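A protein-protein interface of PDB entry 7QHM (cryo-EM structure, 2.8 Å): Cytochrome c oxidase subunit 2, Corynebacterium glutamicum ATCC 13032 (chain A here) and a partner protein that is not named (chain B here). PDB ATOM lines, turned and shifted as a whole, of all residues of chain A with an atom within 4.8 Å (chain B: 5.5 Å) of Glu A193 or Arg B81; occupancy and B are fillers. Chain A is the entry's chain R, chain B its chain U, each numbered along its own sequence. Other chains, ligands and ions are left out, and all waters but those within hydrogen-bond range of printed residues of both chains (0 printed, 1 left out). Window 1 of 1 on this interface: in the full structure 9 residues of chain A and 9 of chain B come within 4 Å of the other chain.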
ATOM      1  N   ASN A 126      -6.005   4.770  41.082  1.00  0.00           N
ATOM      2  CA  ASN A 126      -5.286   3.713  40.382  1.00  0.00           C
ATOM      3  C   ASN A 126      -3.800   3.807  40.716  1.00  0.00           C
ATOM      4  O   ASN A 126      -3.383   4.597  41.569  1.00  0.00           O
ATOM      5  CB  ASN A 126      -5.544   3.790  38.878  1.00  0.00           C
ATOM      6  CG  ASN A 126      -5.695   2.442  38.265  1.00  0.00           C
ATOM      7  OD1 ASN A 126      -4.825   1.598  38.394  1.00  0.00           O
ATOM      8  ND2 ASN A 126      -6.814   2.212  37.609  1.00  0.00           N
ATOM      9  N   GLY A 189      -2.153   2.609  35.278  1.00  0.00           N
ATOM     10  CA  GLY A 189      -3.460   2.004  35.288  1.00  0.00           C
ATOM     11  C   GLY A 189      -4.548   2.997  34.948  1.00  0.00           C
ATOM     12  O   GLY A 189      -4.444   4.190  35.216  1.00  0.00           O
ATOM     13  N   THR A 190      -5.613   2.481  34.342  1.00  0.00           N
ATOM     14  CA  THR A 190      -6.761   3.280  33.949  1.00  0.00           C
ATOM     15  C   THR A 190      -8.022   2.512  34.304  1.00  0.00           C
ATOM     16  O   THR A 190      -7.975   1.333  34.651  1.00  0.00           O
ATOM     17  CB  THR A 190      -6.736   3.616  32.453  1.00  0.00           C
ATOM     18  OG1 THR A 190      -6.837   2.415  31.686  1.00  0.00           O
ATOM     19  CG2 THR A 190      -5.456   4.331  32.082  1.00  0.00           C
ATOM     20  N   THR A 191      -9.160   3.204  34.226  1.00  0.00           N
ATOM     21  CA  THR A 191     -10.447   2.546  34.438  1.00  0.00           C
ATOM     22  C   THR A 191     -10.645   1.385  33.476  1.00  0.00           C
ATOM     23  O   THR A 191     -11.295   0.396  33.828  1.00  0.00           O
ATOM     24  CB  THR A 191     -11.586   3.552  34.276  1.00  0.00           C
ATOM     25  OG1 THR A 191     -11.318   4.716  35.061  1.00  0.00           O
ATOM     26  CG2 THR A 191     -12.902   2.950  34.731  1.00  0.00           C
ATOM     27  N   ASP A 192     -10.077   1.476  32.273  1.00  0.00           N
ATOM     28  CA  ASP A 192     -10.243   0.458  31.254  1.00  0.00           C
ATOM     29  C   ASP A 192      -9.202  -0.652  31.320  1.00  0.00           C
ATOM     30  O   ASP A 192      -9.423  -1.710  30.725  1.00  0.00           O
ATOM     31  CB  ASP A 192     -10.200   1.113  29.870  1.00  0.00           C
ATOM     32  CG  ASP A 192     -10.481   0.128  28.741  1.00  0.00           C
ATOM     33  OD1 ASP A 192     -11.443  -0.663  28.859  1.00  0.00           O
ATOM     34  OD2 ASP A 192      -9.741   0.149  27.735  1.00  0.00           O
ATOM     35  N   GLU A 193      -8.088  -0.459  32.027  1.00  0.00           N
ATOM     36  CA  GLU A 193      -6.990  -1.418  32.013  1.00  0.00           C
ATOM     37  C   GLU A 193      -6.393  -1.592  33.400  1.00  0.00           C
ATOM     38  O   GLU A 193      -6.183  -0.616  34.122  1.00  0.00           O
ATOM     39  CB  GLU A 193      -5.904  -0.972  31.038  1.00  0.00           C
ATOM     40  CG  GLU A 193      -4.760  -1.949  30.901  1.00  0.00           C
ATOM     41  CD  GLU A 193      -3.922  -1.715  29.661  1.00  0.00           C
ATOM     42  OE1 GLU A 193      -4.483  -1.331  28.614  1.00  0.00           O
ATOM     43  OE2 GLU A 193      -2.692  -1.920  29.726  1.00  0.00           O
ATOM     44  N   ILE A 194      -6.109  -2.835  33.760  1.00  0.00           N
ATOM     45  CA  ILE A 194      -5.432  -3.129  35.024  1.00  0.00           C
ATOM     46  C   ILE A 194      -3.927  -2.955  34.822  1.00  0.00           C
ATOM     47  O   ILE A 194      -3.386  -3.479  33.840  1.00  0.00           O
ATOM     48  CB  ILE A 194      -5.758  -4.544  35.492  1.00  0.00           C
ATOM     49  CG1 ILE A 194      -7.229  -4.677  35.881  1.00  0.00           C
ATOM     50  CG2 ILE A 194      -4.857  -4.949  36.640  1.00  0.00           C
ATOM     51  CD1 ILE A 194      -7.666  -3.945  37.138  1.00  0.00           C
ATOM     52  N   PRO A 195      -3.215  -2.244  35.701  1.00  0.00           N
ATOM     53  CA  PRO A 195      -1.756  -2.185  35.563  1.00  0.00           C
ATOM     54  C   PRO A 195      -1.111  -3.484  36.022  1.00  0.00           C
ATOM     55  O   PRO A 195      -1.352  -3.954  37.134  1.00  0.00           O
ATOM     56  CB  PRO A 195      -1.363  -1.015  36.467  1.00  0.00           C
ATOM     57  CG  PRO A 195      -2.409  -0.941  37.452  1.00  0.00           C
ATOM     58  CD  PRO A 195      -3.670  -1.358  36.783  1.00  0.00           C
ATOM     59  N   THR A 294       3.469  -0.162  24.400  1.00  0.00           N
ATOM     60  CA  THR A 294       2.668  -0.242  25.610  1.00  0.00           C
ATOM     61  C   THR A 294       3.089  -1.442  26.454  1.00  0.00           C
ATOM     62  O   THR A 294       4.036  -2.160  26.132  1.00  0.00           O
ATOM     63  CB  THR A 294       1.191  -0.327  25.238  1.00  0.00           C
ATOM     64  OG1 THR A 294       0.955  -1.537  24.514  1.00  0.00           O
ATOM     65  CG2 THR A 294       0.791   0.846  24.368  1.00  0.00           C
ATOM     66  N   ALA A 296       0.991  -4.072  27.288  1.00  0.00           N
ATOM     67  CA  ALA A 296       0.421  -5.285  26.725  1.00  0.00           C
ATOM     68  C   ALA A 296       1.288  -5.828  25.602  1.00  0.00           C
ATOM     69  O   ALA A 296       1.468  -7.045  25.477  1.00  0.00           O
ATOM     70  CB  ALA A 296      -0.989  -5.001  26.221  1.00  0.00           C
ATOM     71  N   TYR A 307      -3.051  -8.774  29.117  1.00  0.00           N
ATOM     72  CA  TYR A 307      -3.800  -8.080  30.150  1.00  0.00           C
ATOM     73  C   TYR A 307      -3.913  -8.962  31.378  1.00  0.00           C
ATOM     74  O   TYR A 307      -3.669 -10.169  31.325  1.00  0.00           O
ATOM     75  CB  TYR A 307      -5.186  -7.685  29.638  1.00  0.00           C
ATOM     76  CG  TYR A 307      -5.118  -6.824  28.410  1.00  0.00           C
ATOM     77  CD1 TYR A 307      -4.783  -5.491  28.500  1.00  0.00           C
ATOM     78  CD2 TYR A 307      -5.374  -7.345  27.163  1.00  0.00           C
ATOM     79  CE1 TYR A 307      -4.705  -4.703  27.381  1.00  0.00           C
ATOM     80  CE2 TYR A 307      -5.296  -6.564  26.037  1.00  0.00           C
ATOM     81  CZ  TYR A 307      -4.963  -5.245  26.154  1.00  0.00           C
ATOM     82  OH  TYR A 307      -4.891  -4.453  25.039  1.00  0.00           O
ATOM     83  N   PRO A 313     -10.732  -5.138  34.935  1.00  0.00           N
ATOM     84  CA  PRO A 313     -11.312  -3.816  35.171  1.00  0.00           C
ATOM     85  C   PRO A 313     -12.810  -3.905  35.384  1.00  0.00           C
ATOM     86  O   PRO A 313     -13.478  -4.832  34.930  1.00  0.00           O
ATOM     87  CB  PRO A 313     -10.978  -3.055  33.889  1.00  0.00           C
ATOM     88  CG  PRO A 313     -10.857  -4.097  32.880  1.00  0.00           C
ATOM     89  CD  PRO A 313     -10.200  -5.227  33.566  1.00  0.00           C
ATOM     90  N   ASN B  51      -7.992   5.935  19.077  1.00  0.00           N
ATOM     91  CA  ASN B  51      -7.926   4.477  18.995  1.00  0.00           C
ATOM     92  C   ASN B  51      -7.783   3.886  20.391  1.00  0.00           C
ATOM     93  O   ASN B  51      -6.877   4.263  21.137  1.00  0.00           O
ATOM     94  CB  ASN B  51      -6.765   4.026  18.116  1.00  0.00           C
ATOM     95  CG  ASN B  51      -6.772   2.537  17.850  1.00  0.00           C
ATOM     96  OD1 ASN B  51      -7.556   1.789  18.422  1.00  0.00           O
ATOM     97  ND2 ASN B  51      -5.889   2.098  16.975  1.00  0.00           N
ATOM     98  N   GLN B  52      -8.679   2.957  20.737  1.00  0.00           N
ATOM     99  CA  GLN B  52      -8.589   2.237  22.000  1.00  0.00           C
ATOM    100  C   GLN B  52      -8.899   0.755  21.816  1.00  0.00           C
ATOM    101  O   GLN B  52      -9.450   0.114  22.715  1.00  0.00           O
ATOM    102  CB  GLN B  52      -9.512   2.852  23.054  1.00  0.00           C
ATOM    103  CG  GLN B  52     -10.969   2.893  22.695  1.00  0.00           C
ATOM    104  CD  GLN B  52     -11.808   3.481  23.802  1.00  0.00           C
ATOM    105  OE1 GLN B  52     -11.320   4.251  24.623  1.00  0.00           O
ATOM    106  NE2 GLN B  52     -13.074   3.107  23.843  1.00  0.00           N
ATOM    107  N   ASP B  53      -8.541   0.197  20.665  1.00  0.00           N
ATOM    108  CA  ASP B  53      -8.764  -1.216  20.409  1.00  0.00           C
ATOM    109  C   ASP B  53      -7.757  -2.040  21.190  1.00  0.00           C
ATOM    110  O   ASP B  53      -6.552  -1.785  21.127  1.00  0.00           O
ATOM    111  CB  ASP B  53      -8.645  -1.493  18.914  1.00  0.00           C
ATOM    112  CG  ASP B  53      -8.560  -2.966  18.594  1.00  0.00           C
ATOM    113  OD1 ASP B  53      -9.558  -3.683  18.803  1.00  0.00           O
ATOM    114  OD2 ASP B  53      -7.498  -3.411  18.119  1.00  0.00           O
ATOM    115  N   THR B  54      -8.247  -3.030  21.931  1.00  0.00           N
ATOM    116  CA  THR B  54      -7.368  -3.849  22.748  1.00  0.00           C
ATOM    117  C   THR B  54      -6.669  -4.945  21.956  1.00  0.00           C
ATOM    118  O   THR B  54      -5.722  -5.546  22.469  1.00  0.00           O
ATOM    119  CB  THR B  54      -8.155  -4.461  23.905  1.00  0.00           C
ATOM    120  OG1 THR B  54      -9.323  -5.117  23.400  1.00  0.00           O
ATOM    121  CG2 THR B  54      -8.572  -3.384  24.883  1.00  0.00           C
ATOM    122  N   HIS B  56      -4.922  -4.197  19.432  1.00  0.00           N
ATOM    123  CA  HIS B  56      -3.749  -3.489  18.919  1.00  0.00           C
ATOM    124  C   HIS B  56      -3.738  -3.420  17.395  1.00  0.00           C
ATOM    125  O   HIS B  56      -2.678  -3.370  16.770  1.00  0.00           O
ATOM    126  CB  HIS B  56      -2.456  -4.109  19.455  1.00  0.00           C
ATOM    127  CG  HIS B  56      -2.262  -3.889  20.921  1.00  0.00           C
ATOM    128  ND1 HIS B  56      -2.482  -4.871  21.860  1.00  0.00           N
ATOM    129  CD2 HIS B  56      -1.892  -2.784  21.613  1.00  0.00           C
ATOM    130  CE1 HIS B  56      -2.248  -4.385  23.064  1.00  0.00           C
ATOM    131  NE2 HIS B  56      -1.885  -3.123  22.942  1.00  0.00           N
ATOM    132  N   ILE B  79      -3.536   5.556  13.473  1.00  0.00           N
ATOM    133  CA  ILE B  79      -3.781   5.783  14.889  1.00  0.00           C
ATOM    134  C   ILE B  79      -3.528   4.456  15.595  1.00  0.00           C
ATOM    135  O   ILE B  79      -4.347   3.539  15.522  1.00  0.00           O
ATOM    136  CB  ILE B  79      -5.200   6.301  15.148  1.00  0.00           C
ATOM    137  CG1 ILE B  79      -5.556   7.442  14.186  1.00  0.00           C
ATOM    138  CG2 ILE B  79      -5.331   6.780  16.593  1.00  0.00           C
ATOM    139  CD1 ILE B  79      -6.944   8.000  14.368  1.00  0.00           C
ATOM    140  N   GLU B  80      -2.391   4.348  16.277  1.00  0.00           N
ATOM    141  CA  GLU B  80      -2.125   3.207  17.139  1.00  0.00           C
ATOM    142  C   GLU B  80      -2.900   3.359  18.442  1.00  0.00           C
ATOM    143  O   GLU B  80      -3.516   4.390  18.699  1.00  0.00           O
ATOM    144  CB  GLU B  80      -0.629   3.074  17.410  1.00  0.00           C
ATOM    145  CG  GLU B  80       0.122   2.277  16.353  1.00  0.00           C
ATOM    146  CD  GLU B  80       0.140   2.960  14.996  1.00  0.00           C
ATOM    147  OE1 GLU B  80       0.379   4.185  14.941  1.00  0.00           O
ATOM    148  OE2 GLU B  80      -0.092   2.272  13.983  1.00  0.00           O
ATOM    149  N   ARG B  81      -2.876   2.322  19.274  1.00  0.00           N
ATOM    150  CA  ARG B  81      -3.687   2.348  20.483  1.00  0.00           C
ATOM    151  C   ARG B  81      -3.239   3.464  21.414  1.00  0.00           C
ATOM    152  O   ARG B  81      -2.045   3.688  21.623  1.00  0.00           O
ATOM    153  CB  ARG B  81      -3.634   1.018  21.226  1.00  0.00           C
ATOM    154  CG  ARG B  81      -4.718   0.912  22.304  1.00  0.00           C
ATOM    155  CD  ARG B  81      -4.670  -0.407  23.033  1.00  0.00           C
ATOM    156  NE  ARG B  81      -3.617  -0.432  24.045  1.00  0.00           N
ATOM    157  CZ  ARG B  81      -3.785  -0.585  25.353  1.00  0.00           C
ATOM    158  NH1 ARG B  81      -4.981  -0.742  25.900  1.00  0.00           N
ATOM    159  NH2 ARG B  81      -2.717  -0.595  26.140  1.00  0.00           N
ATOM    160  N   ASN B  82      -4.220   4.161  21.967  1.00  0.00           N
ATOM    161  CA  ASN B  82      -4.031   5.308  22.840  1.00  0.00           C
ATOM    162  C   ASN B  82      -3.351   6.467  22.125  1.00  0.00           C
ATOM    163  O   ASN B  82      -2.744   7.326  22.769  1.00  0.00           O
ATOM    164  CB  ASN B  82      -3.267   4.924  24.113  1.00  0.00           C
ATOM    165  CG  ASN B  82      -4.023   3.916  24.958  1.00  0.00           C
ATOM    166  OD1 ASN B  82      -5.229   3.746  24.808  1.00  0.00           O
ATOM    167  ND2 ASN B  82      -3.321   3.254  25.856  1.00  0.00           N
ATOM    168  N   CYS B  83      -3.453   6.505  20.799  1.00  0.00           N
ATOM    169  CA  CYS B  83      -3.138   7.681  20.010  1.00  0.00           C
ATOM    170  C   CYS B  83      -4.417   8.409  19.637  1.00  0.00           C
ATOM    171  O   CYS B  83      -5.527   7.842  19.647  1.00  0.00           O
ATOM    172  CB  CYS B  83      -2.377   7.323  18.732  1.00  0.00           C
ATOM    173  SG  CYS B  83      -0.709   6.675  18.986  1.00  0.00           S
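Thr A191 touches none of the printed residues of chain B.
Glu A193 touches just one residue of chain B: Arg B81 (2.8 Å).
Of the printed residues of chain B, Thr A294 touches His B56.
Asn B51 touches none of the printed residues of chain A.
Of the printed residues of chain A, His B56 touches Thr A294, Ala A296 and Tyr A307.
Of the printed residues of chain A, Arg B81 touches Glu A193 (2.8 Å) and Tyr A307 (3.8 Å).
The nearest printed residue of chain A that does not touch Arg B81 is Thr A294 (4.02 Å).
The nearest printed residue of chain B that does not touch Tyr A307 is Asp B53 (5.0 Å).
Of the 10 printed residues of chain B, 3 touch a printed residue of chain A.
Among the printed residues, 6 pairs touch across the chains.
Among the printed residues, Asp or Glu carboxylates within 4 Å of a Lys or Arg side-chain nitrogen of the other chain: Glu A193 with Arg B81 (2.8 Å).
The side-chain hydroxyl (OH) of Tyr A307 lies within hydrogen-bond range of the backbone carbonyl oxygen (O) of Thr B54 (2.9 Å).
The side-chain carboxylate of Glu A193 is in salt-bridge range of the guanidinium group of Arg B81 (2.8 Å).
The backbone carbonyl oxygen (O) of Thr B54 sits at hydrogen-bond distance from a ring nitrogen (ND1) of His B56, 3.4 Å away.
The backbone NH of His B56 sits at hydrogen-bond distance from the side-chain carboxylate of Asp B53, 3.0 Å away.
The guanidinium group (NE) of Arg B81 lies within hydrogen-bond range of a ring nitrogen (NE2) of His B56, at 3.4 Å.
N of Glu A193 lies within hydrogen-bond range of OG1 of Thr A190, 3.2 Å away.
Thr A294 touches His B56.
His B56 touches Ala A296.
Tyr A307 touches His B56 (OH to CE1, 3.3 Å).
NH1 of Arg B81 touches OH of Tyr A307, at 3.8 Å.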
